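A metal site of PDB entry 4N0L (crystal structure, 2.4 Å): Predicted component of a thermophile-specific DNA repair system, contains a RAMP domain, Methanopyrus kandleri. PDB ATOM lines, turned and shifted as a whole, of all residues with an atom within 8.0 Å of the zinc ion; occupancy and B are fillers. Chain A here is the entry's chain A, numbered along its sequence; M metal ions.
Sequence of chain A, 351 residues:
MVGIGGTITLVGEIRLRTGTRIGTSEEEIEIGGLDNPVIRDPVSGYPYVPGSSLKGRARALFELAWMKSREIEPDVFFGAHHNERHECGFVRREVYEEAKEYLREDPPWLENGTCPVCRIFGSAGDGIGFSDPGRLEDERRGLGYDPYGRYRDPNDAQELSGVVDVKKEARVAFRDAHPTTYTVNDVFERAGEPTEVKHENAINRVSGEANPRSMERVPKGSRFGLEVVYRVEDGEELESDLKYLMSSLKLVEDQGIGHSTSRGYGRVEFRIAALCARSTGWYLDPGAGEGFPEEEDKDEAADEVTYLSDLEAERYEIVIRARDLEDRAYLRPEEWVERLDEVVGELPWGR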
ATOM      1  N   ARG A  59       3.593  -0.214 -18.288  1.00  0.00           N
ATOM      2  CA  ARG A  59       4.652   0.018 -19.265  1.00  0.00           C
ATOM      3  C   ARG A  59       4.193   0.907 -20.419  1.00  0.00           C
ATOM      4  O   ARG A  59       4.893   1.835 -20.808  1.00  0.00           O
ATOM      5  CB  ARG A  59       5.163  -1.307 -19.827  1.00  0.00           C
ATOM      6  CG  ARG A  59       6.414  -1.163 -20.684  1.00  0.00           C
ATOM      7  CD  ARG A  59       6.783  -2.471 -21.375  1.00  0.00           C
ATOM      8  NE  ARG A  59       8.158  -2.477 -21.861  1.00  0.00           N
ATOM      9  CZ  ARG A  59       8.590  -1.751 -22.885  1.00  0.00           C
ATOM     10  NH1 ARG A  59       9.864  -1.831 -23.247  1.00  0.00           N
ATOM     11  NH2 ARG A  59       7.776  -0.958 -23.554  1.00  0.00           N
ATOM     12  N   GLU A  63       5.937   4.639 -20.875  1.00  0.00           N
ATOM     13  CA  GLU A  63       6.784   4.905 -22.034  1.00  0.00           C
ATOM     14  C   GLU A  63       6.288   6.143 -22.784  1.00  0.00           C
ATOM     15  O   GLU A  63       7.093   6.948 -23.251  1.00  0.00           O
ATOM     16  CB  GLU A  63       6.843   3.680 -22.960  1.00  0.00           C
ATOM     17  CG  GLU A  63       5.602   3.390 -23.779  1.00  0.00           C
ATOM     18  CD  GLU A  63       5.742   2.133 -24.623  1.00  0.00           C
ATOM     19  OE1 GLU A  63       6.885   1.652 -24.781  1.00  0.00           O
ATOM     20  OE2 GLU A  63       4.727   1.628 -25.135  1.00  0.00           O
ATOM     21  N   TRP A  66       7.155   9.135 -20.539  1.00  0.00           N
ATOM     22  CA  TRP A  66       8.595   9.340 -20.631  1.00  0.00           C
ATOM     23  C   TRP A  66       8.936  10.069 -21.922  1.00  0.00           C
ATOM     24  O   TRP A  66       9.709  11.029 -21.915  1.00  0.00           O
ATOM     25  CB  TRP A  66       9.343   8.011 -20.554  1.00  0.00           C
ATOM     26  CG  TRP A  66      10.840   8.143 -20.530  1.00  0.00           C
ATOM     27  CD1 TRP A  66      11.719   7.722 -21.492  1.00  0.00           C
ATOM     28  CD2 TRP A  66      11.636   8.708 -19.488  1.00  0.00           C
ATOM     29  NE1 TRP A  66      13.007   8.004 -21.112  1.00  0.00           N
ATOM     30  CE2 TRP A  66      12.980   8.612 -19.886  1.00  0.00           C
ATOM     31  CE3 TRP A  66      11.336   9.308 -18.256  1.00  0.00           C
ATOM     32  CZ2 TRP A  66      14.034   9.083 -19.105  1.00  0.00           C
ATOM     33  CZ3 TRP A  66      12.387   9.766 -17.477  1.00  0.00           C
ATOM     34  CH2 TRP A  66      13.716   9.654 -17.896  1.00  0.00           C
ATOM     35  N   PHE A  77      11.431   7.815 -30.827  1.00  0.00           N
ATOM     36  CA  PHE A  77      11.217   7.031 -29.623  1.00  0.00           C
ATOM     37  C   PHE A  77      10.780   5.590 -29.909  1.00  0.00           C
ATOM     38  O   PHE A  77      11.246   4.658 -29.256  1.00  0.00           O
ATOM     39  CB  PHE A  77      10.180   7.716 -28.724  1.00  0.00           C
ATOM     40  CG  PHE A  77      10.018   7.065 -27.385  1.00  0.00           C
ATOM     41  CD1 PHE A  77      11.005   7.186 -26.410  1.00  0.00           C
ATOM     42  CD2 PHE A  77       8.874   6.342 -27.076  1.00  0.00           C
ATOM     43  CE1 PHE A  77      10.862   6.592 -25.170  1.00  0.00           C
ATOM     44  CE2 PHE A  77       8.726   5.742 -25.843  1.00  0.00           C
ATOM     45  CZ  PHE A  77       9.716   5.865 -24.885  1.00  0.00           C
ATOM     46  N   HIS A  86       8.020   0.712 -27.207  1.00  0.00           N
ATOM     47  CA  HIS A  86       9.425   1.098 -27.311  1.00  0.00           C
ATOM     48  C   HIS A  86      10.290   0.003 -26.706  1.00  0.00           C
ATOM     49  O   HIS A  86      10.067  -0.403 -25.567  1.00  0.00           O
ATOM     50  CB  HIS A  86       9.691   2.435 -26.603  1.00  0.00           C
ATOM     51  CG  HIS A  86      11.126   2.624 -26.210  1.00  0.00           C
ATOM     52  ND1 HIS A  86      12.027   3.325 -26.978  1.00  0.00           N
ATOM     53  CD2 HIS A  86      11.813   2.215 -25.103  1.00  0.00           C
ATOM     54  CE1 HIS A  86      13.209   3.339 -26.382  1.00  0.00           C
ATOM     55  NE2 HIS A  86      13.102   2.673 -25.240  1.00  0.00           N
ATOM     56  N   GLU A  87      11.257  -0.472 -27.475  1.00  0.00           N
ATOM     57  CA  GLU A  87      12.217  -1.435 -26.962  1.00  0.00           C
ATOM     58  C   GLU A  87      13.629  -1.099 -27.432  1.00  0.00           C
ATOM     59  O   GLU A  87      13.871  -0.986 -28.633  1.00  0.00           O
ATOM     60  CB  GLU A  87      11.838  -2.854 -27.389  1.00  0.00           C
ATOM     61  CG  GLU A  87      10.603  -3.402 -26.709  1.00  0.00           C
ATOM     62  CD  GLU A  87      10.197  -4.758 -27.236  1.00  0.00           C
ATOM     63  OE1 GLU A  87       9.762  -4.840 -28.402  1.00  0.00           O
ATOM     64  OE2 GLU A  87      10.312  -5.744 -26.488  1.00  0.00           O
ATOM     65  N   CYS A  88      14.542  -0.924 -26.489  1.00  0.00           N
ATOM     66  CA  CYS A  88      15.941  -0.675 -26.815  1.00  0.00           C
ATOM     67  C   CYS A  88      16.828  -1.555 -25.945  1.00  0.00           C
ATOM     68  O   CYS A  88      16.352  -2.173 -24.987  1.00  0.00           O
ATOM     69  CB  CYS A  88      16.300   0.799 -26.628  1.00  0.00           C
ATOM     70  SG  CYS A  88      16.539   1.308 -24.910  1.00  0.00           S
ATOM     71  N   GLY A  89      18.112  -1.592 -26.262  1.00  0.00           N
ATOM     72  CA  GLY A  89      19.044  -2.432 -25.523  1.00  0.00           C
ATOM     73  C   GLY A  89      19.888  -1.652 -24.547  1.00  0.00           C
ATOM     74  O   GLY A  89      20.758  -2.216 -23.888  1.00  0.00           O
ATOM     75  N   PHE A  90      19.635  -0.350 -24.429  1.00  0.00           N
ATOM     76  CA  PHE A  90      20.370   0.479 -23.486  1.00  0.00           C
ATOM     77  C   PHE A  90      19.864   0.223 -22.069  1.00  0.00           C
ATOM     78  O   PHE A  90      19.317   1.119 -21.418  1.00  0.00           O
ATOM     79  CB  PHE A  90      20.226   1.967 -23.837  1.00  0.00           C
ATOM     80  CG  PHE A  90      20.849   2.347 -25.143  1.00  0.00           C
ATOM     81  CD1 PHE A  90      22.215   2.629 -25.214  1.00  0.00           C
ATOM     82  CD2 PHE A  90      20.094   2.441 -26.294  1.00  0.00           C
ATOM     83  CE1 PHE A  90      22.796   2.980 -26.412  1.00  0.00           C
ATOM     84  CE2 PHE A  90      20.678   2.792 -27.509  1.00  0.00           C
ATOM     85  CZ  PHE A  90      22.027   3.070 -27.565  1.00  0.00           C
ATOM     86  N   VAL A  91      20.061  -0.993 -21.574  1.00  0.00           N
ATOM     87  CA  VAL A  91      19.436  -1.440 -20.331  1.00  0.00           C
ATOM     88  C   VAL A  91      20.417  -1.502 -19.158  1.00  0.00           C
ATOM     89  O   VAL A  91      20.004  -1.606 -18.003  1.00  0.00           O
ATOM     90  CB  VAL A  91      18.793  -2.822 -20.508  1.00  0.00           C
ATOM     91  CG1 VAL A  91      17.585  -2.718 -21.430  1.00  0.00           C
ATOM     92  CG2 VAL A  91      19.796  -3.811 -21.058  1.00  0.00           C
ATOM     93  N   TRP A 109      16.076   9.529 -24.937  1.00  0.00           N
ATOM     94  CA  TRP A 109      15.284   8.797 -23.964  1.00  0.00           C
ATOM     95  C   TRP A 109      16.182   8.131 -22.920  1.00  0.00           C
ATOM     96  O   TRP A 109      15.734   7.297 -22.147  1.00  0.00           O
ATOM     97  CB  TRP A 109      14.410   7.733 -24.634  1.00  0.00           C
ATOM     98  CG  TRP A 109      15.198   6.646 -25.292  1.00  0.00           C
ATOM     99  CD1 TRP A 109      15.663   5.509 -24.711  1.00  0.00           C
ATOM    100  CD2 TRP A 109      15.598   6.588 -26.671  1.00  0.00           C
ATOM    101  NE1 TRP A 109      16.340   4.740 -25.631  1.00  0.00           N
ATOM    102  CE2 TRP A 109      16.316   5.384 -26.838  1.00  0.00           C
ATOM    103  CE3 TRP A 109      15.427   7.435 -27.761  1.00  0.00           C
ATOM    104  CZ2 TRP A 109      16.857   5.013 -28.078  1.00  0.00           C
ATOM    105  CZ3 TRP A 109      15.964   7.063 -28.984  1.00  0.00           C
ATOM    106  CH2 TRP A 109      16.671   5.860 -29.129  1.00  0.00           C
ATOM    107  N   LEU A 110      17.457   8.510 -22.917  1.00  0.00           N
ATOM    108  CA  LEU A 110      18.418   7.923 -22.004  1.00  0.00           C
ATOM    109  C   LEU A 110      18.607   8.816 -20.769  1.00  0.00           C
ATOM    110  O   LEU A 110      18.556  10.045 -20.874  1.00  0.00           O
ATOM    111  CB  LEU A 110      19.761   7.706 -22.710  1.00  0.00           C
ATOM    112  CG  LEU A 110      19.855   6.460 -23.602  1.00  0.00           C
ATOM    113  CD1 LEU A 110      21.304   6.163 -23.978  1.00  0.00           C
ATOM    114  CD2 LEU A 110      19.208   5.257 -22.929  1.00  0.00           C
ATOM    115  N   THR A 114      21.274   4.895 -19.434  1.00  0.00           N
ATOM    116  CA  THR A 114      20.359   3.771 -19.535  1.00  0.00           C
ATOM    117  C   THR A 114      18.913   4.199 -19.743  1.00  0.00           C
ATOM    118  O   THR A 114      18.537   5.341 -19.463  1.00  0.00           O
ATOM    119  CB  THR A 114      20.413   2.865 -18.293  1.00  0.00           C
ATOM    120  OG1 THR A 114      20.056   3.621 -17.126  1.00  0.00           O
ATOM    121  CG2 THR A 114      21.813   2.282 -18.109  1.00  0.00           C
ATOM    122  N   CYS A 115      18.098   3.269 -20.243  1.00  0.00           N
ATOM    123  CA  CYS A 115      16.688   3.540 -20.514  1.00  0.00           C
ATOM    124  C   CYS A 115      15.815   3.040 -19.375  1.00  0.00           C
ATOM    125  O   CYS A 115      15.761   1.845 -19.110  1.00  0.00           O
ATOM    126  CB  CYS A 115      16.265   2.874 -21.833  1.00  0.00           C
ATOM    127  SG  CYS A 115      14.582   3.249 -22.367  1.00  0.00           S
ATOM    128  N   PRO A 116      15.115   3.968 -18.701  1.00  0.00           N
ATOM    129  CA  PRO A 116      14.208   3.650 -17.591  1.00  0.00           C
ATOM    130  C   PRO A 116      13.097   2.690 -18.009  1.00  0.00           C
ATOM    131  O   PRO A 116      12.785   1.755 -17.266  1.00  0.00           O
ATOM    132  CB  PRO A 116      13.630   5.012 -17.197  1.00  0.00           C
ATOM    133  CG  PRO A 116      14.628   6.001 -17.678  1.00  0.00           C
ATOM    134  CD  PRO A 116      15.194   5.426 -18.939  1.00  0.00           C
ATOM    135  N   VAL A 117      12.497   2.932 -19.164  1.00  0.00           N
ATOM    136  CA  VAL A 117      11.438   2.079 -19.683  1.00  0.00           C
ATOM    137  C   VAL A 117      11.859   0.625 -19.787  1.00  0.00           C
ATOM    138  O   VAL A 117      11.242  -0.261 -19.187  1.00  0.00           O
ATOM    139  CB  VAL A 117      10.960   2.543 -21.073  1.00  0.00           C
ATOM    140  CG1 VAL A 117       9.918   1.586 -21.624  1.00  0.00           C
ATOM    141  CG2 VAL A 117      10.420   3.968 -21.008  1.00  0.00           C
ATOM    142  N   CYS A 118      12.920   0.381 -20.537  1.00  0.00           N
ATOM    143  CA  CYS A 118      13.362  -0.975 -20.843  1.00  0.00           C
ATOM    144  C   CYS A 118      14.071  -1.671 -19.663  1.00  0.00           C
ATOM    145  O   CYS A 118      13.907  -2.871 -19.476  1.00  0.00           O
ATOM    146  CB  CYS A 118      14.279  -0.964 -22.070  1.00  0.00           C
ATOM    147  SG  CYS A 118      13.414  -0.502 -23.609  1.00  0.00           S
ATOM    148  N   ARG A 119      14.832  -0.920 -18.879  1.00  0.00           N
ATOM    149  CA  ARG A 119      15.557  -1.518 -17.755  1.00  0.00           C
ATOM    150  C   ARG A 119      14.601  -1.971 -16.639  1.00  0.00           C
ATOM    151  O   ARG A 119      14.883  -2.926 -15.914  1.00  0.00           O
ATOM    152  CB  ARG A 119      16.612  -0.558 -17.201  1.00  0.00           C
ATOM    153  CG  ARG A 119      16.080   0.457 -16.193  1.00  0.00           C
ATOM    154  CD  ARG A 119      17.026   1.629 -16.007  1.00  0.00           C
ATOM    155  NE  ARG A 119      16.561   2.516 -14.950  1.00  0.00           N
ATOM    156  CZ  ARG A 119      16.879   3.804 -14.852  1.00  0.00           C
ATOM    157  NH1 ARG A 119      17.675   4.372 -15.747  1.00  0.00           N
ATOM    158  NH2 ARG A 119      16.397   4.532 -13.849  1.00  0.00           N
ATOM    159  N   GLY A 122      11.513  -4.315 -18.888  1.00  0.00           N
ATOM    160  CA  GLY A 122      12.046  -5.327 -19.784  1.00  0.00           C
ATOM    161  C   GLY A 122      12.046  -4.892 -21.235  1.00  0.00           C
ATOM    162  O   GLY A 122      11.400  -3.907 -21.593  1.00  0.00           O
ATOM    163  N   SER A 123      12.765  -5.631 -22.064  1.00  0.00           N
ATOM    164  CA  SER A 123      12.836  -5.350 -23.489  1.00  0.00           C
ATOM    165  C   SER A 123      13.337  -6.576 -24.246  1.00  0.00           C
ATOM    166  O   SER A 123      14.163  -7.333 -23.725  1.00  0.00           O
ATOM    167  CB  SER A 123      13.758  -4.157 -23.758  1.00  0.00           C
ATOM    168  OG  SER A 123      13.922  -3.922 -25.141  1.00  0.00           O
ATOM    169  N   GLY A 125      15.044  -6.362 -26.915  1.00  0.00           N
ATOM    170  CA  GLY A 125      16.291  -5.952 -27.514  1.00  0.00           C
ATOM    171  C   GLY A 125      16.147  -4.641 -28.258  1.00  0.00           C
ATOM    172  O   GLY A 125      15.517  -3.712 -27.760  1.00  0.00           O
ATOM    173  N   ILE A 128      13.117  -1.111 -31.600  1.00  0.00           N
ATOM    174  CA  ILE A 128      12.918   0.115 -32.370  1.00  0.00           C
ATOM    175  C   ILE A 128      13.800   0.130 -33.621  1.00  0.00           C
ATOM    176  O   ILE A 128      13.563   0.911 -34.544  1.00  0.00           O
ATOM    177  CB  ILE A 128      13.209   1.372 -31.534  1.00  0.00           C
ATOM    178  CG1 ILE A 128      14.642   1.355 -31.014  1.00  0.00           C
ATOM    179  CG2 ILE A 128      12.230   1.473 -30.363  1.00  0.00           C
ATOM    180  CD1 ILE A 128      15.015   2.570 -30.202  1.00  0.00           C
HETATM  181 ZN    ZN M   1      14.318   1.616 -23.991  1.00  0.00          ZN
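N of Phe 90 lies close to SG of Cys 88, at 3.5 Å.
The side-chain sulfur (SG) of Cys 88 sits close to the indole nitrogen (NE1) of Trp 109 (3.5 Å).
N of His 86 is in hydrogen-bond range of OE1 of Glu 63 (2.8 Å).
The backbone carbonyl oxygen of Phe 77 lies within hydrogen-bond range of a ring nitrogen (ND1) of His 86 (2.8 Å).
The backbone NH of Cys 115 lies within hydrogen-bond range of the backbone carbonyl oxygen of Phe 90, at 2.7 Å.
SG of Cys 118 sits close to OG of Ser 123 (3.8 Å).
O of Cys 88 lies within hydrogen-bond range of OG of Ser 123 (3.0 Å).
O of His 86 sits at hydrogen-bond distance from NH1 of Arg 59.
Of the 22 residues printed, 4 come within 4 Å of the zinc ion.
The nearest printed residue that does not touch the zinc ion is Trp 109 (4.1 Å).
The zinc ion is bound by a ring nitrogen (NE2) of His 86 (2.0 Å), the side-chain sulfur of Cys 115 (2.3 Å), the side-chain sulfur of Cys 118 (2.3 Å) and the side-chain sulfur of Cys 88 (2.4 Å).
The zinc ion has four donor atoms within binding distance.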
